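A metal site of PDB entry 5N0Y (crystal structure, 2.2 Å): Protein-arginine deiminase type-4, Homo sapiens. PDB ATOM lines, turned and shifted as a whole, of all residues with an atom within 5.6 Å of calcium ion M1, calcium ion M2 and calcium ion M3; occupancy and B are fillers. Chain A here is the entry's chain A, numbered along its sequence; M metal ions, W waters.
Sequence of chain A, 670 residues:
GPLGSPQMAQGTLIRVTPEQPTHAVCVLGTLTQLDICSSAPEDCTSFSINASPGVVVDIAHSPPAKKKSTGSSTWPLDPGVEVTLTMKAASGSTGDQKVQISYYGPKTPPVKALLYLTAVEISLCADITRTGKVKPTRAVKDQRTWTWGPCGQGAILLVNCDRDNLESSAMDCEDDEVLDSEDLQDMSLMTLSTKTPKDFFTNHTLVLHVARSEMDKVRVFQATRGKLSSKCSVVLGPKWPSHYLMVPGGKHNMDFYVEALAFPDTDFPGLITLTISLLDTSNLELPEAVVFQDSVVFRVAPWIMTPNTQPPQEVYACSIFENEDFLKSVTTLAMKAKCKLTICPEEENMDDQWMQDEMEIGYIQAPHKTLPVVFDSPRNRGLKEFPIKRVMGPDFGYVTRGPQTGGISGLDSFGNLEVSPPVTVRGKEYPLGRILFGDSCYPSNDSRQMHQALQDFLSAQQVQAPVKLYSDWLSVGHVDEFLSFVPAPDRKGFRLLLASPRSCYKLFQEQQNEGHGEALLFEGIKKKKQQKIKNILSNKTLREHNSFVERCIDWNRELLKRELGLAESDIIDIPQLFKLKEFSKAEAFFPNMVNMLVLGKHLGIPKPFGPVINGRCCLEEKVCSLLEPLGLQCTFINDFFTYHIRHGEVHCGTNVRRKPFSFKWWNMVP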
ATOM      1  N   ASN A 160     -16.965   1.884  30.133  1.00  0.00           N
ATOM      2  CA  ASN A 160     -16.773   1.683  28.690  1.00  0.00           C
ATOM      3  C   ASN A 160     -17.769   0.631  28.219  1.00  0.00           C
ATOM      4  O   ASN A 160     -17.420  -0.467  27.834  1.00  0.00           O
ATOM      5  CB  ASN A 160     -15.306   1.337  28.410  1.00  0.00           C
ATOM      6  CG  ASN A 160     -14.930   1.428  26.935  1.00  0.00           C
ATOM      7  OD1 ASN A 160     -15.698   1.908  26.121  1.00  0.00           O
ATOM      8  ND2 ASN A 160     -13.746   0.939  26.598  1.00  0.00           N
ATOM      9  N   ASP A 162     -20.273   1.108  25.802  1.00  0.00           N
ATOM     10  CA  ASP A 162     -20.678   1.087  24.380  1.00  0.00           C
ATOM     11  C   ASP A 162     -19.972  -0.060  23.609  1.00  0.00           C
ATOM     12  O   ASP A 162     -19.345  -0.970  24.220  1.00  0.00           O
ATOM     13  CB  ASP A 162     -20.492   2.489  23.723  1.00  0.00           C
ATOM     14  CG  ASP A 162     -19.034   2.842  23.514  1.00  0.00           C
ATOM     15  OD1 ASP A 162     -18.186   2.073  24.014  1.00  0.00           O
ATOM     16  OD2 ASP A 162     -18.740   3.901  22.891  1.00  0.00           O
ATOM     17  N   ARG A 163     -20.104  -0.027  22.273  1.00  0.00           N
ATOM     18  CA  ARG A 163     -19.518  -1.040  21.359  1.00  0.00           C
ATOM     19  C   ARG A 163     -19.039  -0.320  20.097  1.00  0.00           C
ATOM     20  O   ARG A 163     -19.710  -0.321  19.059  1.00  0.00           O
ATOM     21  CB  ARG A 163     -20.526  -2.126  21.060  1.00  0.00           C
ATOM     22  CG  ARG A 163     -20.210  -3.085  19.921  1.00  0.00           C
ATOM     23  CD  ARG A 163     -21.286  -4.162  19.813  1.00  0.00           C
ATOM     24  NE  ARG A 163     -22.622  -3.686  19.352  1.00  0.00           N
ATOM     25  CZ  ARG A 163     -23.810  -4.189  19.749  1.00  0.00           C
ATOM     26  NH1 ARG A 163     -23.907  -5.198  20.617  1.00  0.00           N
ATOM     27  NH2 ARG A 163     -24.951  -3.671  19.289  1.00  0.00           N
ATOM     28  N   ASP A 164     -17.898   0.367  20.243  1.00  0.00           N
ATOM     29  CA  ASP A 164     -17.121   0.886  19.118  1.00  0.00           C
ATOM     30  C   ASP A 164     -16.613  -0.239  18.143  1.00  0.00           C
ATOM     31  O   ASP A 164     -16.402   0.022  16.953  1.00  0.00           O
ATOM     32  CB  ASP A 164     -15.940   1.703  19.619  1.00  0.00           C
ATOM     33  CG  ASP A 164     -16.348   3.005  20.239  1.00  0.00           C
ATOM     34  OD1 ASP A 164     -17.127   3.767  19.621  1.00  0.00           O
ATOM     35  OD2 ASP A 164     -15.852   3.307  21.347  1.00  0.00           O
ATOM     36  N   ASP A 172     -17.363  -2.953  24.786  1.00  0.00           N
ATOM     37  CA  ASP A 172     -15.886  -2.844  24.705  1.00  0.00           C
ATOM     38  C   ASP A 172     -15.100  -3.348  25.920  1.00  0.00           C
ATOM     39  O   ASP A 172     -14.027  -3.949  25.736  1.00  0.00           O
ATOM     40  CB  ASP A 172     -15.481  -1.405  24.413  1.00  0.00           C
ATOM     41  CG  ASP A 172     -15.992  -0.922  23.096  1.00  0.00           C
ATOM     42  OD1 ASP A 172     -16.311  -1.762  22.187  1.00  0.00           O
ATOM     43  OD2 ASP A 172     -16.049   0.315  22.957  1.00  0.00           O
ATOM     44  N   CYS A 173     -15.626  -3.127  27.138  1.00  0.00           N
ATOM     45  CA  CYS A 173     -14.881  -3.386  28.385  1.00  0.00           C
ATOM     46  C   CYS A 173     -14.975  -4.839  28.887  1.00  0.00           C
ATOM     47  O   CYS A 173     -14.437  -5.169  29.969  1.00  0.00           O
ATOM     48  CB  CYS A 173     -15.388  -2.450  29.485  1.00  0.00           C
ATOM     49  SG  CYS A 173     -17.099  -2.740  30.026  1.00  0.00           S
ATOM     50  N   GLU A 174     -15.682  -5.705  28.148  1.00  0.00           N
ATOM     51  CA  GLU A 174     -15.730  -7.127  28.556  1.00  0.00           C
ATOM     52  C   GLU A 174     -14.448  -7.990  28.256  1.00  0.00           C
ATOM     53  O   GLU A 174     -14.238  -8.979  28.891  1.00  0.00           O
ATOM     54  CB  GLU A 174     -17.044  -7.771  28.114  1.00  0.00           C
ATOM     55  CG  GLU A 174     -18.173  -7.392  29.085  1.00  0.00           C
ATOM     56  CD  GLU A 174     -19.587  -7.544  28.555  1.00  0.00           C
ATOM     57  OE1 GLU A 174     -19.754  -7.766  27.332  1.00  0.00           O
ATOM     58  OE2 GLU A 174     -20.549  -7.450  29.356  1.00  0.00           O
ATOM     59  N   ASP A 175     -13.562  -7.569  27.380  1.00  0.00           N
ATOM     60  CA  ASP A 175     -12.347  -8.339  27.074  1.00  0.00           C
ATOM     61  C   ASP A 175     -11.173  -7.604  27.733  1.00  0.00           C
ATOM     62  O   ASP A 175     -11.386  -6.571  28.392  1.00  0.00           O
ATOM     63  CB  ASP A 175     -12.156  -8.453  25.541  1.00  0.00           C
ATOM     64  CG  ASP A 175     -11.884  -7.098  24.867  1.00  0.00           C
ATOM     65  OD1 ASP A 175     -11.762  -6.062  25.579  1.00  0.00           O
ATOM     66  OD2 ASP A 175     -11.818  -7.053  23.609  1.00  0.00           O
ATOM     67  N   ASP A 176      -9.950  -8.126  27.506  1.00  0.00           N
ATOM     68  CA  ASP A 176      -8.682  -7.532  27.994  1.00  0.00           C
ATOM     69  C   ASP A 176      -7.837  -6.835  26.918  1.00  0.00           C
ATOM     70  O   ASP A 176      -6.610  -6.840  27.013  1.00  0.00           O
ATOM     71  CB  ASP A 176      -7.844  -8.605  28.704  1.00  0.00           C
ATOM     72  CG  ASP A 176      -8.531  -9.174  29.947  1.00  0.00           C
ATOM     73  OD1 ASP A 176      -8.623  -8.485  30.996  1.00  0.00           O
ATOM     74  OD2 ASP A 176      -8.973 -10.338  29.882  1.00  0.00           O
ATOM     75  N   GLU A 177      -8.476  -6.217  25.922  1.00  0.00           N
ATOM     76  CA  GLU A 177      -7.768  -5.541  24.821  1.00  0.00           C
ATOM     77  C   GLU A 177      -8.498  -4.286  24.323  1.00  0.00           C
ATOM     78  O   GLU A 177      -9.734  -4.189  24.433  1.00  0.00           O
ATOM     79  CB  GLU A 177      -7.580  -6.471  23.584  1.00  0.00           C
ATOM     80  CG  GLU A 177      -7.535  -7.970  23.851  1.00  0.00           C
ATOM     81  CD  GLU A 177      -7.282  -8.811  22.608  1.00  0.00           C
ATOM     82  OE1 GLU A 177      -6.434  -8.447  21.765  1.00  0.00           O
ATOM     83  OE2 GLU A 177      -7.932  -9.877  22.488  1.00  0.00           O
ATOM     84  N   VAL A 178      -7.719  -3.377  23.727  1.00  0.00           N
ATOM     85  CA  VAL A 178      -8.201  -2.220  22.993  1.00  0.00           C
ATOM     86  C   VAL A 178      -8.144  -2.587  21.526  1.00  0.00           C
ATOM     87  O   VAL A 178      -7.058  -2.573  20.935  1.00  0.00           O
ATOM     88  CB  VAL A 178      -7.285  -1.003  23.187  1.00  0.00           C
ATOM     89  CG1 VAL A 178      -7.791   0.219  22.413  1.00  0.00           C
ATOM     90  CG2 VAL A 178      -7.120  -0.703  24.663  1.00  0.00           C
ATOM     91  N   LEU A 179      -9.302  -2.885  20.935  1.00  0.00           N
ATOM     92  CA  LEU A 179      -9.390  -3.386  19.558  1.00  0.00           C
ATOM     93  C   LEU A 179      -9.561  -2.327  18.485  1.00  0.00           C
ATOM     94  O   LEU A 179      -9.320  -2.635  17.351  1.00  0.00           O
ATOM     95  CB  LEU A 179     -10.544  -4.379  19.435  1.00  0.00           C
ATOM     96  CG  LEU A 179     -10.348  -5.673  20.207  1.00  0.00           C
ATOM     97  CD1 LEU A 179     -11.605  -6.518  20.036  1.00  0.00           C
ATOM     98  CD2 LEU A 179      -9.096  -6.419  19.755  1.00  0.00           C
ATOM     99  N   GLU A 182     -10.441   4.311  18.205  1.00  0.00           N
ATOM    100  CA  GLU A 182     -11.592   5.093  18.640  1.00  0.00           C
ATOM    101  C   GLU A 182     -11.960   4.795  20.108  1.00  0.00           C
ATOM    102  O   GLU A 182     -12.277   5.714  20.847  1.00  0.00           O
ATOM    103  CB  GLU A 182     -12.823   4.775  17.761  1.00  0.00           C
ATOM    104  CG  GLU A 182     -12.818   5.348  16.334  1.00  0.00           C
ATOM    105  CD  GLU A 182     -12.104   4.479  15.293  1.00  0.00           C
ATOM    106  OE1 GLU A 182     -11.804   5.042  14.225  1.00  0.00           O
ATOM    107  OE2 GLU A 182     -11.827   3.269  15.519  1.00  0.00           O
ATOM    108  N   ASP A 183     -11.913   3.516  20.489  1.00  0.00           N
ATOM    109  CA  ASP A 183     -12.178   3.061  21.843  1.00  0.00           C
ATOM    110  C   ASP A 183     -11.441   3.921  22.869  1.00  0.00           C
ATOM    111  O   ASP A 183     -12.043   4.283  23.898  1.00  0.00           O
ATOM    112  CB  ASP A 183     -11.822   1.575  22.022  1.00  0.00           C
ATOM    113  CG  ASP A 183     -12.415   0.956  23.299  1.00  0.00           C
ATOM    114  OD1 ASP A 183     -13.512   1.346  23.700  1.00  0.00           O
ATOM    115  OD2 ASP A 183     -11.788   0.016  23.860  1.00  0.00           O
ATOM    116  N   ASP A 186     -13.002   6.962  24.708  1.00  0.00           N
ATOM    117  CA  ASP A 186     -13.854   6.698  25.842  1.00  0.00           C
ATOM    118  C   ASP A 186     -13.076   6.657  27.156  1.00  0.00           C
ATOM    119  O   ASP A 186     -13.662   6.855  28.209  1.00  0.00           O
ATOM    120  CB  ASP A 186     -14.611   5.392  25.651  1.00  0.00           C
ATOM    121  CG  ASP A 186     -15.522   5.415  24.458  1.00  0.00           C
ATOM    122  OD1 ASP A 186     -16.035   6.500  24.088  1.00  0.00           O
ATOM    123  OD2 ASP A 186     -15.736   4.333  23.875  1.00  0.00           O
ATOM    124  N   PHE A 221      -4.585   0.257  30.725  1.00  0.00           N
ATOM    125  CA  PHE A 221      -3.760  -0.119  29.583  1.00  0.00           C
ATOM    126  C   PHE A 221      -2.538   0.747  29.493  1.00  0.00           C
ATOM    127  O   PHE A 221      -2.658   1.979  29.636  1.00  0.00           O
ATOM    128  CB  PHE A 221      -4.527   0.072  28.289  1.00  0.00           C
ATOM    129  CG  PHE A 221      -5.657  -0.880  28.120  1.00  0.00           C
ATOM    130  CD1 PHE A 221      -5.419  -2.188  27.631  1.00  0.00           C
ATOM    131  CD2 PHE A 221      -6.966  -0.480  28.410  1.00  0.00           C
ATOM    132  CE1 PHE A 221      -6.488  -3.068  27.441  1.00  0.00           C
ATOM    133  CE2 PHE A 221      -8.009  -1.372  28.255  1.00  0.00           C
ATOM    134  CZ  PHE A 221      -7.770  -2.661  27.771  1.00  0.00           C
ATOM    135  N   GLU A 259     -10.267   2.478  31.829  1.00  0.00           N
ATOM    136  CA  GLU A 259     -11.704   2.312  31.635  1.00  0.00           C
ATOM    137  C   GLU A 259     -12.317   1.719  32.902  1.00  0.00           C
ATOM    138  O   GLU A 259     -11.666   0.936  33.608  1.00  0.00           O
ATOM    139  CB  GLU A 259     -12.010   1.374  30.423  1.00  0.00           C
ATOM    140  CG  GLU A 259     -11.356  -0.021  30.537  1.00  0.00           C
ATOM    141  CD  GLU A 259     -11.646  -1.005  29.373  1.00  0.00           C
ATOM    142  OE1 GLU A 259     -12.229  -0.561  28.351  1.00  0.00           O
ATOM    143  OE2 GLU A 259     -11.288  -2.235  29.486  1.00  0.00           O
ATOM    144  N   LYS A 369     -15.511  13.330  26.988  1.00  0.00           N
ATOM    145  CA  LYS A 369     -16.411  12.429  26.261  1.00  0.00           C
ATOM    146  C   LYS A 369     -17.777  12.308  26.972  1.00  0.00           C
ATOM    147  O   LYS A 369     -17.837  12.128  28.192  1.00  0.00           O
ATOM    148  CB  LYS A 369     -15.771  11.050  26.118  1.00  0.00           C
ATOM    149  CG  LYS A 369     -16.618   9.977  25.513  1.00  0.00           C
ATOM    150  CD  LYS A 369     -17.071  10.321  24.106  1.00  0.00           C
ATOM    151  CE  LYS A 369     -16.032  10.070  23.038  1.00  0.00           C
ATOM    152  NZ  LYS A 369     -16.704  10.018  21.724  1.00  0.00           N
ATOM    153  N   LEU A 371     -21.607  10.376  26.164  1.00  0.00           N
ATOM    154  CA  LEU A 371     -22.314   9.537  25.244  1.00  0.00           C
ATOM    155  C   LEU A 371     -23.611   8.991  25.846  1.00  0.00           C
ATOM    156  O   LEU A 371     -23.724   8.878  27.030  1.00  0.00           O
ATOM    157  CB  LEU A 371     -21.405   8.427  24.808  1.00  0.00           C
ATOM    158  CG  LEU A 371     -20.930   7.467  25.902  1.00  0.00           C
ATOM    159  CD1 LEU A 371     -21.558   6.122  25.647  1.00  0.00           C
ATOM    160  CD2 LEU A 371     -19.428   7.259  25.949  1.00  0.00           C
ATOM    161  N   PRO A 394     -21.634   1.998  18.379  1.00  0.00           N
ATOM    162  CA  PRO A 394     -20.595   3.022  18.467  1.00  0.00           C
ATOM    163  C   PRO A 394     -21.121   4.263  19.130  1.00  0.00           C
ATOM    164  O   PRO A 394     -22.052   4.876  18.621  1.00  0.00           O
ATOM    165  CB  PRO A 394     -20.231   3.303  16.984  1.00  0.00           C
ATOM    166  CG  PRO A 394     -20.753   2.130  16.235  1.00  0.00           C
ATOM    167  CD  PRO A 394     -21.930   1.592  16.999  1.00  0.00           C
ATOM    168  N   ASP A 395     -20.528   4.636  20.243  1.00  0.00           N
ATOM    169  CA  ASP A 395     -20.932   5.856  20.975  1.00  0.00           C
ATOM    170  C   ASP A 395     -22.359   5.799  21.546  1.00  0.00           C
ATOM    171  O   ASP A 395     -22.972   6.815  21.792  1.00  0.00           O
ATOM    172  CB  ASP A 395     -20.621   7.124  20.145  1.00  0.00           C
ATOM    173  CG  ASP A 395     -19.150   7.501  20.235  1.00  0.00           C
ATOM    174  OD1 ASP A 395     -18.372   6.663  20.705  1.00  0.00           O
ATOM    175  OD2 ASP A 395     -18.742   8.632  19.887  1.00  0.00           O
HETATM  176 CA    CA M   1     -15.768   2.197  23.671  1.00  0.00          CA
HETATM  177 CA    CA M   2     -17.008   5.389  21.979  1.00  0.00          CA
HETATM  178 CA    CA M   3     -11.833  -3.951  25.089  1.00  0.00          CA
HETATM  179  O   HOH W   1     -15.245   6.013  20.820  1.00  0.00           O
HETATM  180  O   HOH W   2     -12.737  -4.315  22.957  1.00  0.00           O
HETATM  181  O   HOH W   3     -11.331  -4.371  27.434  1.00  0.00           O
HETATM  182  O   HOH W   4     -11.740  -1.725  25.834  1.00  0.00           O
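OD2 of Asp 172 binds calcium ion M1 (2.0 Å).
OD2 of Asp 186 binds calcium ion M1 (2.1 Å).
The side-chain carboxylate (OD1) of Asp 183 is bound to calcium ion M1 (2.4 Å).
The side-chain carboxylate (OD1) of Asp 162 is bound to calcium ion M1 (2.4 Å).
Calcium ion M1 is bound by OD1 of Asn 160, 2.5 Å away.
The side-chain carboxylate (OD2) of Asp 164 is bound to calcium ion M1, at 2.6 Å.
Calcium ion M2 is bound by water W1 (2.2 Å), the side-chain carboxylate (OD1) of Asp 395 (2.3 Å), the side-chain carboxylate (OD2) of Asp 162 (2.5 Å), the side-chain carboxylate (OD2) of Asp 164 (2.5 Å), the side-chain carboxylate (OD2) of Asp 186 (2.5 Å), the side-chain carboxylate (OD1) of Asp 186 (2.6 Å) and the side-chain carboxylate (OD1) of Asp 164 (2.9 Å).
Calcium ion M2 has seven donor atoms within binding distance.
Water W4 lies within hydrogen-bond range of OD2 of Asp 183, OE1 of Glu 259 and ND2 of Asn 160.
Water W3 lies within hydrogen-bond range of O of Asp 175 (2.4 Å) and OE2 of Glu 259 (3.0 Å).
Of the 21 residues printed, 3 come within 4 Å of calcium ion M3.
The nearest printed residue that does not touch calcium ion M3 is Asp 183 (4.2 Å).
Of the 21 residues printed, 6 come within 4 Å of calcium ion M1.
The nearest printed residue that does not touch calcium ion M1 is Arg 163 (5.1 Å).
Calcium ion M3 is bound by the side-chain carboxylate of Asp 175 (2.2 Å), the backbone carbonyl oxygen of Glu 177 (2.2 Å), the backbone carbonyl oxygen of Asp 172 (2.3 Å), water W2 (2.3 Å), water W4 (2.3 Å) and water W3 (2.4 Å).
Calcium ion M3 has six donor atoms within binding distance.
Four residues have an atom within 4 Å of calcium ion M2: Asp 162, Asp 164, Asp 186 and Asp 395.
The nearest printed residue that does not touch calcium ion M2 is Lys 369 (4.6 Å).
The backbone carbonyl oxygen (O) of Asn 160 sits at hydrogen-bond distance from the side-chain sulfur (SG) of Cys 173 (3.2 Å).
The side-chain amide nitrogen of Asn 160 lies within hydrogen-bond range of the side-chain carboxylate of Glu 259 (2.8 Å).
The side-chain carboxylate (OD2) of Asp 395 is in salt-bridge range of the side-chain amino group (NZ) of Lys 369 (3.1 Å).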
